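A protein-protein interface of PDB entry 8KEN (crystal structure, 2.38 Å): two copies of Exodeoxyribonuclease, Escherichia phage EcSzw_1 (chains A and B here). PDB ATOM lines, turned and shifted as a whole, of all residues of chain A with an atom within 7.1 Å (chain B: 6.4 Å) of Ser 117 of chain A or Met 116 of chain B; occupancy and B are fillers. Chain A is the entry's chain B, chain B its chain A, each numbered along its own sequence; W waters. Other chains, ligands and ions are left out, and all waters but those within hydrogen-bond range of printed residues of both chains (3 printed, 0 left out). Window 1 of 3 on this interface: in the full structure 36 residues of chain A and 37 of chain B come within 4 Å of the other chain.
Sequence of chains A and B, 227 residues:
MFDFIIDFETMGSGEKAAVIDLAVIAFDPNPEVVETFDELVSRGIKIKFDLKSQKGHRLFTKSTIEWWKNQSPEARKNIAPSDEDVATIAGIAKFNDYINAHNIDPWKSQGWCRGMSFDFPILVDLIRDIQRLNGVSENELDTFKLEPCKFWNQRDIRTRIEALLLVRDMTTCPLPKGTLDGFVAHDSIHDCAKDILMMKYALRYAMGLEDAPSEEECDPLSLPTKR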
ATOM      1  N   SER A  13      -9.899  12.171 -11.251  1.00  0.00           N
ATOM      2  CA  SER A  13      -8.519  12.419 -11.642  1.00  0.00           C
ATOM      3  C   SER A  13      -8.371  13.585 -12.607  1.00  0.00           C
ATOM      4  O   SER A  13      -7.501  14.443 -12.405  1.00  0.00           O
ATOM      5  CB  SER A  13      -7.908  11.152 -12.286  1.00  0.00           C
ATOM      6  OG  SER A  13      -8.014  10.018 -11.432  1.00  0.00           O
ATOM      7  N   GLY A  14      -9.149  13.639 -13.678  1.00  0.00           N
ATOM      8  CA  GLY A  14      -8.942  14.686 -14.662  1.00  0.00           C
ATOM      9  C   GLY A  14      -9.533  16.042 -14.259  1.00  0.00           C
ATOM     10  O   GLY A  14      -9.906  16.289 -13.110  1.00  0.00           O
ATOM     11  N   GLU A  15      -9.616  16.936 -15.252  1.00  0.00           N
ATOM     12  CA  GLU A  15     -10.165  18.275 -15.031  1.00  0.00           C
ATOM     13  C   GLU A  15     -11.667  18.248 -14.766  1.00  0.00           C
ATOM     14  O   GLU A  15     -12.195  19.198 -14.183  1.00  0.00           O
ATOM     15  CB  GLU A  15      -9.846  19.191 -16.227  1.00  0.00           C
ATOM     16  CG  GLU A  15     -10.860  19.151 -17.382  1.00  0.00           C
ATOM     17  CD  GLU A  15     -10.347  19.807 -18.680  1.00  0.00           C
ATOM     18  OE1 GLU A  15      -9.179  20.267 -18.725  1.00  0.00           O
ATOM     19  OE2 GLU A  15     -11.128  19.889 -19.655  1.00  0.00           O
ATOM     20  N   CYS A 113      -0.712  25.547  -5.593  1.00  0.00           N
ATOM     21  CA  CYS A 113      -1.293  24.261  -5.201  1.00  0.00           C
ATOM     22  C   CYS A 113      -0.230  23.173  -5.258  1.00  0.00           C
ATOM     23  O   CYS A 113       0.775  23.295  -5.960  1.00  0.00           O
ATOM     24  CB  CYS A 113      -2.484  23.865  -6.086  1.00  0.00           C
ATOM     25  SG  CYS A 113      -1.978  23.427  -7.761  1.00  0.00           S
ATOM     26  N   ARG A 114      -0.463  22.101  -4.494  1.00  0.00           N
ATOM     27  CA  ARG A 114       0.463  20.958  -4.442  1.00  0.00           C
ATOM     28  C   ARG A 114       0.222  20.053  -5.654  1.00  0.00           C
ATOM     29  O   ARG A 114      -0.478  19.038  -5.595  1.00  0.00           O
ATOM     30  CB  ARG A 114       0.311  20.180  -3.138  1.00  0.00           C
ATOM     31  CG  ARG A 114       1.459  19.177  -2.917  1.00  0.00           C
ATOM     32  CD  ARG A 114       1.480  18.630  -1.491  1.00  0.00           C
ATOM     33  NE  ARG A 114       2.119  19.575  -0.576  1.00  0.00           N
ATOM     34  CZ  ARG A 114       3.428  19.702  -0.414  1.00  0.00           C
ATOM     35  NH1 ARG A 114       4.279  18.889  -1.019  1.00  0.00           N
ATOM     36  NH2 ARG A 114       3.895  20.664   0.381  1.00  0.00           N
ATOM     37  N   GLY A 115       0.806  20.430  -6.784  1.00  0.00           N
ATOM     38  CA  GLY A 115       0.532  19.674  -7.986  1.00  0.00           C
ATOM     39  C   GLY A 115      -0.239  20.495  -8.986  1.00  0.00           C
ATOM     40  O   GLY A 115      -1.455  20.325  -9.125  1.00  0.00           O
ATOM     41  N   MET A 116       0.474  21.371  -9.699  1.00  0.00           N
ATOM     42  CA  MET A 116      -0.169  22.357 -10.556  1.00  0.00           C
ATOM     43  C   MET A 116      -1.106  21.739 -11.581  1.00  0.00           C
ATOM     44  O   MET A 116      -2.130  22.341 -11.927  1.00  0.00           O
ATOM     45  CB  MET A 116       0.894  23.201 -11.252  1.00  0.00           C
ATOM     46  CG  MET A 116       0.787  24.688 -10.908  1.00  0.00           C
ATOM     47  SD  MET A 116       2.091  25.638 -11.681  1.00  0.00           S
ATOM     48  CE  MET A 116       1.488  25.747 -13.357  1.00  0.00           C
ATOM     49  N   SER A 117      -0.783  20.554 -12.085  1.00  0.00           N
ATOM     50  CA  SER A 117      -1.633  19.901 -13.078  1.00  0.00           C
ATOM     51  C   SER A 117      -2.893  19.289 -12.470  1.00  0.00           C
ATOM     52  O   SER A 117      -3.725  18.748 -13.202  1.00  0.00           O
ATOM     53  CB  SER A 117      -0.847  18.801 -13.805  1.00  0.00           C
ATOM     54  OG  SER A 117      -0.412  17.829 -12.861  1.00  0.00           O
ATOM     55  N   PHE A 118      -3.051  19.328 -11.157  1.00  0.00           N
ATOM     56  CA  PHE A 118      -4.237  18.715 -10.588  1.00  0.00           C
ATOM     57  C   PHE A 118      -5.310  19.761 -10.277  1.00  0.00           C
ATOM     58  O   PHE A 118      -6.380  19.756 -10.900  1.00  0.00           O
ATOM     59  CB  PHE A 118      -3.848  17.911  -9.351  1.00  0.00           C
ATOM     60  CG  PHE A 118      -4.975  17.135  -8.773  1.00  0.00           C
ATOM     61  CD1 PHE A 118      -5.291  15.877  -9.265  1.00  0.00           C
ATOM     62  CD2 PHE A 118      -5.739  17.673  -7.736  1.00  0.00           C
ATOM     63  CE1 PHE A 118      -6.358  15.144  -8.717  1.00  0.00           C
ATOM     64  CE2 PHE A 118      -6.804  16.959  -7.192  1.00  0.00           C
ATOM     65  CZ  PHE A 118      -7.122  15.685  -7.688  1.00  0.00           C
ATOM     66  N   ASP A 119      -5.023  20.696  -9.357  1.00  0.00           N
ATOM     67  CA  ASP A 119      -6.064  21.622  -8.898  1.00  0.00           C
ATOM     68  C   ASP A 119      -6.386  22.701  -9.918  1.00  0.00           C
ATOM     69  O   ASP A 119      -7.563  23.016 -10.132  1.00  0.00           O
ATOM     70  CB  ASP A 119      -5.667  22.253  -7.576  1.00  0.00           C
ATOM     71  CG  ASP A 119      -5.213  21.216  -6.591  1.00  0.00           C
ATOM     72  OD1 ASP A 119      -4.067  20.753  -6.727  1.00  0.00           O
ATOM     73  OD2 ASP A 119      -6.023  20.818  -5.728  1.00  0.00           O
ATOM     74  N   PHE A 120      -5.382  23.290 -10.549  1.00  0.00           N
ATOM     75  CA  PHE A 120      -5.748  24.401 -11.424  1.00  0.00           C
ATOM     76  C   PHE A 120      -6.617  23.982 -12.611  1.00  0.00           C
ATOM     77  O   PHE A 120      -7.509  24.748 -12.984  1.00  0.00           O
ATOM     78  CB  PHE A 120      -4.499  25.150 -11.887  1.00  0.00           C
ATOM     79  CG  PHE A 120      -4.055  26.181 -10.894  1.00  0.00           C
ATOM     80  CD1 PHE A 120      -4.846  27.318 -10.656  1.00  0.00           C
ATOM     81  CD2 PHE A 120      -2.904  25.990 -10.135  1.00  0.00           C
ATOM     82  CE1 PHE A 120      -4.474  28.260  -9.706  1.00  0.00           C
ATOM     83  CE2 PHE A 120      -2.518  26.923  -9.190  1.00  0.00           C
ATOM     84  CZ  PHE A 120      -3.308  28.070  -8.969  1.00  0.00           C
ATOM     85  N   PRO A 121      -6.424  22.806 -13.235  1.00  0.00           N
ATOM     86  CA  PRO A 121      -7.359  22.425 -14.309  1.00  0.00           C
ATOM     87  C   PRO A 121      -8.765  22.181 -13.807  1.00  0.00           C
ATOM     88  O   PRO A 121      -9.717  22.431 -14.549  1.00  0.00           O
ATOM     89  CB  PRO A 121      -6.730  21.149 -14.897  1.00  0.00           C
ATOM     90  CG  PRO A 121      -5.280  21.347 -14.644  1.00  0.00           C
ATOM     91  CD  PRO A 121      -5.216  21.951 -13.267  1.00  0.00           C
ATOM     92  N   ILE A 122      -8.933  21.711 -12.570  1.00  0.00           N
ATOM     93  CA  ILE A 122     -10.279  21.546 -12.027  1.00  0.00           C
ATOM     94  C   ILE A 122     -10.896  22.904 -11.700  1.00  0.00           C
ATOM     95  O   ILE A 122     -12.080  23.153 -11.979  1.00  0.00           O
ATOM     96  CB  ILE A 122     -10.253  20.625 -10.796  1.00  0.00           C
ATOM     97  CG1 ILE A 122      -9.920  19.169 -11.193  1.00  0.00           C
ATOM     98  CG2 ILE A 122     -11.565  20.683 -10.070  1.00  0.00           C
ATOM     99  CD1 ILE A 122      -9.338  18.344 -10.029  1.00  0.00           C
ATOM    100  N   GLN A 154       0.433  30.866 -12.245  1.00  0.00           N
ATOM    101  CA  GLN A 154       0.250  29.663 -11.447  1.00  0.00           C
ATOM    102  C   GLN A 154       1.620  29.114 -11.056  1.00  0.00           C
ATOM    103  O   GLN A 154       2.580  29.208 -11.824  1.00  0.00           O
ATOM    104  CB  GLN A 154      -0.560  28.622 -12.218  1.00  0.00           C
ATOM    105  CG  GLN A 154      -2.002  29.043 -12.560  1.00  0.00           C
ATOM    106  CD  GLN A 154      -2.678  28.041 -13.486  1.00  0.00           C
ATOM    107  OE1 GLN A 154      -2.265  26.897 -13.562  1.00  0.00           O
ATOM    108  NE2 GLN A 154      -3.687  28.480 -14.215  1.00  0.00           N
ATOM    109  N   ASP A 156       3.797  25.995  -8.536  1.00  0.00           N
ATOM    110  CA  ASP A 156       3.702  24.637  -8.014  1.00  0.00           C
ATOM    111  C   ASP A 156       4.475  24.519  -6.710  1.00  0.00           C
ATOM    112  O   ASP A 156       5.665  24.848  -6.651  1.00  0.00           O
ATOM    113  CB  ASP A 156       4.232  23.612  -9.018  1.00  0.00           C
ATOM    114  CG  ASP A 156       4.188  22.204  -8.473  1.00  0.00           C
ATOM    115  OD1 ASP A 156       3.067  21.686  -8.240  1.00  0.00           O
ATOM    116  OD2 ASP A 156       5.273  21.617  -8.284  1.00  0.00           O
ATOM    117  N   ARG A 158       5.362  21.783  -4.906  1.00  0.00           N
ATOM    118  CA  ARG A 158       6.431  20.786  -4.890  1.00  0.00           C
ATOM    119  C   ARG A 158       7.702  21.325  -5.525  1.00  0.00           C
ATOM    120  O   ARG A 158       8.802  21.125  -5.001  1.00  0.00           O
ATOM    121  CB  ARG A 158       5.991  19.520  -5.623  1.00  0.00           C
ATOM    122  CG  ARG A 158       5.018  18.686  -4.872  1.00  0.00           C
ATOM    123  CD  ARG A 158       4.905  17.382  -5.529  1.00  0.00           C
ATOM    124  NE  ARG A 158       3.762  16.629  -5.038  1.00  0.00           N
ATOM    125  CZ  ARG A 158       2.646  16.433  -5.719  1.00  0.00           C
ATOM    126  NH1 ARG A 158       2.473  16.958  -6.921  1.00  0.00           N
ATOM    127  NH2 ARG A 158       1.700  15.659  -5.198  1.00  0.00           N
ATOM    128  N   THR A 159       7.570  21.998  -6.669  1.00  0.00           N
ATOM    129  CA  THR A 159       8.738  22.543  -7.352  1.00  0.00           C
ATOM    130  C   THR A 159       9.395  23.633  -6.510  1.00  0.00           C
ATOM    131  O   THR A 159      10.628  23.681  -6.403  1.00  0.00           O
ATOM    132  CB  THR A 159       8.330  23.075  -8.732  1.00  0.00           C
ATOM    133  OG1 THR A 159       7.502  22.107  -9.402  1.00  0.00           O
ATOM    134  CG2 THR A 159       9.556  23.355  -9.586  1.00  0.00           C
ATOM    135  N   GLY B 111       9.391  15.019 -14.829  1.00  0.00           N
ATOM    136  CA  GLY B 111       8.952  15.609 -16.093  1.00  0.00           C
ATOM    137  C   GLY B 111       8.674  17.091 -15.922  1.00  0.00           C
ATOM    138  O   GLY B 111       8.085  17.503 -14.921  1.00  0.00           O
ATOM    139  N   TRP B 112       9.101  17.890 -16.905  1.00  0.00           N
ATOM    140  CA  TRP B 112       9.091  19.347 -16.808  1.00  0.00           C
ATOM    141  C   TRP B 112       8.355  19.934 -18.003  1.00  0.00           C
ATOM    142  O   TRP B 112       8.476  19.425 -19.126  1.00  0.00           O
ATOM    143  CB  TRP B 112      10.527  19.962 -16.776  1.00  0.00           C
ATOM    144  CG  TRP B 112      11.387  19.563 -15.600  1.00  0.00           C
ATOM    145  CD1 TRP B 112      12.141  18.414 -15.480  1.00  0.00           C
ATOM    146  CD2 TRP B 112      11.616  20.318 -14.399  1.00  0.00           C
ATOM    147  NE1 TRP B 112      12.788  18.405 -14.261  1.00  0.00           N
ATOM    148  CE2 TRP B 112      12.487  19.558 -13.583  1.00  0.00           C
ATOM    149  CE3 TRP B 112      11.169  21.561 -13.933  1.00  0.00           C
ATOM    150  CZ2 TRP B 112      12.913  20.000 -12.323  1.00  0.00           C
ATOM    151  CZ3 TRP B 112      11.600  22.004 -12.678  1.00  0.00           C
ATOM    152  CH2 TRP B 112      12.461  21.224 -11.890  1.00  0.00           C
ATOM    153  N   CYS B 113       7.631  21.033 -17.756  1.00  0.00           N
ATOM    154  CA  CYS B 113       7.024  21.823 -18.821  1.00  0.00           C
ATOM    155  C   CYS B 113       6.843  23.249 -18.325  1.00  0.00           C
ATOM    156  O   CYS B 113       6.885  23.515 -17.119  1.00  0.00           O
ATOM    157  CB  CYS B 113       5.690  21.224 -19.279  1.00  0.00           C
ATOM    158  SG  CYS B 113       4.341  21.470 -18.103  1.00  0.00           S
ATOM    159  N   ARG B 114       6.655  24.168 -19.278  1.00  0.00           N
ATOM    160  CA  ARG B 114       6.519  25.595 -18.974  1.00  0.00           C
ATOM    161  C   ARG B 114       5.061  25.916 -18.651  1.00  0.00           C
ATOM    162  O   ARG B 114       4.346  26.582 -19.408  1.00  0.00           O
ATOM    163  CB  ARG B 114       7.035  26.453 -20.122  1.00  0.00           C
ATOM    164  CG  ARG B 114       7.135  27.947 -19.734  1.00  0.00           C
ATOM    165  CD  ARG B 114       8.041  28.734 -20.665  1.00  0.00           C
ATOM    166  NE  ARG B 114       9.443  28.678 -20.269  1.00  0.00           N
ATOM    167  CZ  ARG B 114      10.006  29.492 -19.381  1.00  0.00           C
ATOM    168  NH1 ARG B 114       9.303  30.417 -18.750  1.00  0.00           N
ATOM    169  NH2 ARG B 114      11.306  29.373 -19.120  1.00  0.00           N
ATOM    170  N   GLY B 115       4.649  25.475 -17.462  1.00  0.00           N
ATOM    171  CA  GLY B 115       3.269  25.607 -17.025  1.00  0.00           C
ATOM    172  C   GLY B 115       2.660  24.231 -16.866  1.00  0.00           C
ATOM    173  O   GLY B 115       2.079  23.708 -17.821  1.00  0.00           O
ATOM    174  N   MET B 116       2.827  23.620 -15.685  1.00  0.00           N
ATOM    175  CA  MET B 116       2.377  22.245 -15.478  1.00  0.00           C
ATOM    176  C   MET B 116       0.906  22.074 -15.817  1.00  0.00           C
ATOM    177  O   MET B 116       0.499  21.029 -16.342  1.00  0.00           O
ATOM    178  CB  MET B 116       2.612  21.807 -14.030  1.00  0.00           C
ATOM    179  CG  MET B 116       3.818  20.929 -13.793  1.00  0.00           C
ATOM    180  SD  MET B 116       4.149  20.702 -12.023  1.00  0.00           S
ATOM    181  CE  MET B 116       2.705  19.730 -11.559  1.00  0.00           C
ATOM    182  N   SER B 117       0.084  23.075 -15.505  1.00  0.00           N
ATOM    183  CA  SER B 117      -1.348  22.935 -15.730  1.00  0.00           C
ATOM    184  C   SER B 117      -1.700  22.918 -17.208  1.00  0.00           C
ATOM    185  O   SER B 117      -2.860  22.696 -17.557  1.00  0.00           O
ATOM    186  CB  SER B 117      -2.107  24.072 -15.044  1.00  0.00           C
ATOM    187  OG  SER B 117      -1.569  25.320 -15.444  1.00  0.00           O
ATOM    188  N   PHE B 118      -0.749  23.168 -18.095  1.00  0.00           N
ATOM    189  CA  PHE B 118      -1.085  23.166 -19.507  1.00  0.00           C
ATOM    190  C   PHE B 118      -0.658  21.868 -20.207  1.00  0.00           C
ATOM    191  O   PHE B 118      -1.511  21.178 -20.763  1.00  0.00           O
ATOM    192  CB  PHE B 118      -0.499  24.416 -20.182  1.00  0.00           C
ATOM    193  CG  PHE B 118      -0.941  24.573 -21.610  1.00  0.00           C
ATOM    194  CD1 PHE B 118      -0.235  23.952 -22.646  1.00  0.00           C
ATOM    195  CD2 PHE B 118      -2.063  25.318 -21.918  1.00  0.00           C
ATOM    196  CE1 PHE B 118      -0.656  24.087 -23.964  1.00  0.00           C
ATOM    197  CE2 PHE B 118      -2.487  25.444 -23.233  1.00  0.00           C
ATOM    198  CZ  PHE B 118      -1.795  24.833 -24.259  1.00  0.00           C
ATOM    199  N   ASP B 119       0.631  21.502 -20.176  1.00  0.00           N
ATOM    200  CA  ASP B 119       1.104  20.375 -21.011  1.00  0.00           C
ATOM    201  C   ASP B 119       0.761  19.014 -20.415  1.00  0.00           C
ATOM    202  O   ASP B 119       0.220  18.146 -21.103  1.00  0.00           O
ATOM    203  CB  ASP B 119       2.610  20.468 -21.234  1.00  0.00           C
ATOM    204  CG  ASP B 119       2.995  21.778 -21.873  1.00  0.00           C
ATOM    205  OD1 ASP B 119       3.240  22.726 -21.088  1.00  0.00           O
ATOM    206  OD2 ASP B 119       3.011  21.864 -23.135  1.00  0.00           O
ATOM    207  N   PHE B 120       1.045  18.826 -19.137  1.00  0.00           N
ATOM    208  CA  PHE B 120       0.760  17.547 -18.503  1.00  0.00           C
ATOM    209  C   PHE B 120      -0.701  17.122 -18.562  1.00  0.00           C
ATOM    210  O   PHE B 120      -0.941  15.924 -18.777  1.00  0.00           O
ATOM    211  CB  PHE B 120       1.312  17.564 -17.066  1.00  0.00           C
ATOM    212  CG  PHE B 120       2.785  17.247 -17.021  1.00  0.00           C
ATOM    213  CD1 PHE B 120       3.244  15.969 -17.404  1.00  0.00           C
ATOM    214  CD2 PHE B 120       3.716  18.224 -16.701  1.00  0.00           C
ATOM    215  CE1 PHE B 120       4.611  15.674 -17.411  1.00  0.00           C
ATOM    216  CE2 PHE B 120       5.079  17.939 -16.705  1.00  0.00           C
ATOM    217  CZ  PHE B 120       5.528  16.666 -17.053  1.00  0.00           C
ATOM    218  N   PRO B 121      -1.707  17.987 -18.358  1.00  0.00           N
ATOM    219  CA  PRO B 121      -3.090  17.485 -18.507  1.00  0.00           C
ATOM    220  C   PRO B 121      -3.419  17.039 -19.924  1.00  0.00           C
ATOM    221  O   PRO B 121      -4.133  16.049 -20.111  1.00  0.00           O
ATOM    222  CB  PRO B 121      -3.946  18.672 -18.057  1.00  0.00           C
ATOM    223  CG  PRO B 121      -3.063  19.401 -17.060  1.00  0.00           C
ATOM    224  CD  PRO B 121      -1.677  19.305 -17.684  1.00  0.00           C
ATOM    225  N   PHE B 151       3.021  11.189 -10.990  1.00  0.00           N
ATOM    226  CA  PHE B 151       2.403  12.512 -11.035  1.00  0.00           C
ATOM    227  C   PHE B 151       3.066  13.454 -10.039  1.00  0.00           C
ATOM    228  O   PHE B 151       3.343  14.612 -10.370  1.00  0.00           O
ATOM    229  CB  PHE B 151       0.875  12.447 -10.846  1.00  0.00           C
ATOM    230  CG  PHE B 151       0.406  11.994  -9.486  1.00  0.00           C
ATOM    231  CD1 PHE B 151       0.240  12.915  -8.442  1.00  0.00           C
ATOM    232  CD2 PHE B 151       0.018  10.680  -9.278  1.00  0.00           C
ATOM    233  CE1 PHE B 151      -0.231  12.514  -7.179  1.00  0.00           C
ATOM    234  CE2 PHE B 151      -0.467  10.264  -8.033  1.00  0.00           C
ATOM    235  CZ  PHE B 151      -0.593  11.180  -6.980  1.00  0.00           C
ATOM    236  N   GLN B 154       6.008  15.445 -11.613  1.00  0.00           N
ATOM    237  CA  GLN B 154       5.941  16.539 -12.560  1.00  0.00           C
ATOM    238  C   GLN B 154       6.484  17.789 -11.879  1.00  0.00           C
ATOM    239  O   GLN B 154       6.452  17.906 -10.654  1.00  0.00           O
ATOM    240  CB  GLN B 154       4.510  16.755 -13.046  1.00  0.00           C
ATOM    241  CG  GLN B 154       3.882  15.553 -13.712  1.00  0.00           C
ATOM    242  CD  GLN B 154       2.365  15.686 -13.844  1.00  0.00           C
ATOM    243  OE1 GLN B 154       1.814  16.772 -13.693  1.00  0.00           O
ATOM    244  NE2 GLN B 154       1.688  14.579 -14.124  1.00  0.00           N
ATOM    245  N   ARG B 155       7.036  18.704 -12.679  1.00  0.00           N
ATOM    246  CA  ARG B 155       7.719  19.866 -12.142  1.00  0.00           C
ATOM    247  C   ARG B 155       7.460  21.041 -13.069  1.00  0.00           C
ATOM    248  O   ARG B 155       7.381  20.860 -14.286  1.00  0.00           O
ATOM    249  CB  ARG B 155       9.222  19.598 -11.987  1.00  0.00           C
ATOM    250  CG  ARG B 155       9.587  18.606 -10.877  1.00  0.00           C
ATOM    251  CD  ARG B 155       9.416  19.234  -9.500  1.00  0.00           C
ATOM    252  NE  ARG B 155       9.843  18.357  -8.408  1.00  0.00           N
ATOM    253  CZ  ARG B 155       9.139  17.338  -7.924  1.00  0.00           C
ATOM    254  NH1 ARG B 155       7.944  17.023  -8.408  1.00  0.00           N
ATOM    255  NH2 ARG B 155       9.641  16.617  -6.923  1.00  0.00           N
ATOM    256  N   ASP B 156       7.291  22.235 -12.491  1.00  0.00           N
ATOM    257  CA  ASP B 156       6.950  23.424 -13.261  1.00  0.00           C
ATOM    258  C   ASP B 156       8.182  24.286 -13.492  1.00  0.00           C
ATOM    259  O   ASP B 156       8.893  24.629 -12.539  1.00  0.00           O
ATOM    260  CB  ASP B 156       5.868  24.249 -12.574  1.00  0.00           C
ATOM    261  CG  ASP B 156       5.518  25.475 -13.363  1.00  0.00           C
ATOM    262  OD1 ASP B 156       5.078  25.324 -14.527  1.00  0.00           O
ATOM    263  OD2 ASP B 156       5.702  26.591 -12.830  1.00  0.00           O
ATOM    264  N   ILE B 157       8.408  24.656 -14.761  1.00  0.00           N
ATOM    265  CA  ILE B 157       9.629  25.366 -15.153  1.00  0.00           C
ATOM    266  C   ILE B 157       9.643  26.794 -14.603  1.00  0.00           C
ATOM    267  O   ILE B 157      10.670  27.264 -14.101  1.00  0.00           O
ATOM    268  CB  ILE B 157       9.780  25.350 -16.687  1.00  0.00           C
ATOM    269  CG1 ILE B 157      10.158  23.953 -17.173  1.00  0.00           C
ATOM    270  CG2 ILE B 157      10.815  26.377 -17.159  1.00  0.00           C
ATOM    271  CD1 ILE B 157      10.129  23.816 -18.669  1.00  0.00           C
ATOM    272  N   ARG B 158       8.519  27.510 -14.715  1.00  0.00           N
ATOM    273  CA  ARG B 158       8.444  28.871 -14.186  1.00  0.00           C
ATOM    274  C   ARG B 158       8.767  28.898 -12.696  1.00  0.00           C
ATOM    275  O   ARG B 158       9.526  29.756 -12.220  1.00  0.00           O
ATOM    276  CB  ARG B 158       7.053  29.459 -14.438  1.00  0.00           C
ATOM    277  CG  ARG B 158       6.778  29.894 -15.872  1.00  0.00           C
ATOM    278  CD  ARG B 158       5.430  30.584 -15.966  1.00  0.00           C
ATOM    279  NE  ARG B 158       4.927  30.669 -17.333  1.00  0.00           N
ATOM    280  CZ  ARG B 158       3.883  29.986 -17.789  1.00  0.00           C
ATOM    281  NH1 ARG B 158       3.225  29.131 -17.024  1.00  0.00           N
ATOM    282  NH2 ARG B 158       3.492  30.162 -19.045  1.00  0.00           N
HETATM  283  O   HOH W   1       0.853  16.243  -9.829  1.00  0.00           O
HETATM  284  O   HOH W   2       3.682  28.290 -13.933  1.00  0.00           O
HETATM  285  O   HOH W   3       4.531  18.658  -8.549  1.00  0.00           O
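OG of Ser 117 of chain A lies within hydrogen-bond range of OE1 of Gln 154 of chain B (2.6 Å).
OE1 of Gln 154 of chain A is in hydrogen-bond range of OG of Ser 117 of chain B, 2.6 Å away.
The side-chain hydroxyl (OG1) of Thr 159 of chain A is in hydrogen-bond range of the backbone NH (N) of Asp 156 of chain B.
The side-chain carboxylate of Asp 156 of chain A is in hydrogen-bond range of the backbone NH of Arg 158 of chain A (3.4 Å).
OD2 of Asp 156 of chain A lies within hydrogen-bond range of OG1 of Thr 159 of chain A, at 2.5 Å.
The backbone NH of Arg 155 of chain B sits at hydrogen-bond distance from the backbone carbonyl oxygen of Gly 111 of chain B, 2.8 Å away.
SG of Cys 113 of chain B lies close to N of Met 116 of chain B (3.6 Å).
N of Gly 115 of chain B lies within hydrogen-bond range of OD1 of Asp 156 of chain B, at 3.0 Å.
The side-chain sulfur (SD) of Met 116 of chain B sits close to the backbone NH (N) of Arg 155 of chain B (3.6 Å).
Of the 17 printed residues of chain A, 7 touch a printed residue of chain B.
Hydrophobic or aromatic side chains of chain A within 4 Å of the printed part of chain B: Met 116 and Pro 121.
Along chain A the printed residues that touch a printed residue of chain B span positions 115 to 159.
Of the 17 printed residues of chain B, 8 touch a printed residue of chain A.
Hydrophobic or aromatic side chains of chain B that line the printed part of chain A: Trp 112, Met 116 and Pro 121.
Among the printed residues, no Asp or Glu carboxylate lies within 4 Å of a Lys or Arg side-chain nitrogen of the other chain.
Met 116 of chain A touches Asp 156 of chain B, and with the chains exchanged Asp 156 of chain A touches Met 116 of chain B.
Ser 117 of chain A touches Pro 121 of chain B, but with the chains exchanged Pro 121 of chain A does not touch Ser 117 of chain B (4.02 Å).
Ser 117 of chain A touches Gln 154 of chain B, and with the chains exchanged Gln 154 of chain A touches Ser 117 of chain B.
Pro 121 of chain B touches its own counterpart, Pro 121 of chain A.
12 positions are printed for both chains.
Of chain B, only Met 116 (3.6 Å), Pro 121 (3.97 Å) and Gln 154 (2.6 Å) come within 4 Å of Ser 117 of chain A.
Printed residues of chain A within 4 Å of Met 116 of chain B: Gly 115 (3.98 Å), Met 116 (3.3 Å), Ser 117 (3.6 Å) and Asp 156 (3.9 Å).
Printed residues of chain B within 4 Å of Gln 154 of chain A: Ser 117 (2.6 Å).
Of the printed residues of chain A, Trp 112 of chain B touches Thr 159 (3.9 Å).
Arg 114 of chain A touches none of the printed residues of chain B.
The nearest residue of chain B that does not touch Ser 117 of chain A is Ser 117 of chain B (4.04 Å).
Water W2 lies within hydrogen-bond range of the backbone carbonyl oxygen (O) of Gln 154 of chain A (2.6 Å), the side-chain carboxylate (OD2) of Asp 156 of chain B (2.9 Å) and the guanidinium group (NH1) of Arg 158 of chain B (3.2 Å).
Water W3 lies within hydrogen-bond range of the backbone carbonyl oxygen (O) of Gln 154 of chain B (2.9 Å), the side-chain carboxylate (OD2) of Asp 156 of chain A (3.1 Å) and the guanidinium group (NH1) of Arg 158 of chain A (3.1 Å).
Water W1 lies within hydrogen-bond range of O of Phe 151 of chain B (3.0 Å) and NH1 of Arg 158 of chain A (3.4 Å).
C of Gly 115 of chain B touches CE of Met 116 of chain A, at 3.998 Å.
Met 116 of chain A touches Met 116 of chain B (N to CE, 3.3 Å).
Met 116 of chain A touches Ser 117 of chain B.
Met 116 of chain A touches Asp 156 of chain B.
Met 116 of chain B touches Ser 117 of chain A.
Pro 121 of chain B touches Ser 117 of chain A.
CG of Pro 121 of chain A touches CG of Pro 121 of chain B, 3.8 Å away.
Asp 156 of chain A touches Met 116 of chain B.
CB of Asp 156 of chain A touches CB of Asp 156 of chain B, 3.97 Å away.
Thr 159 of chain A touches Trp 112 of chain B.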
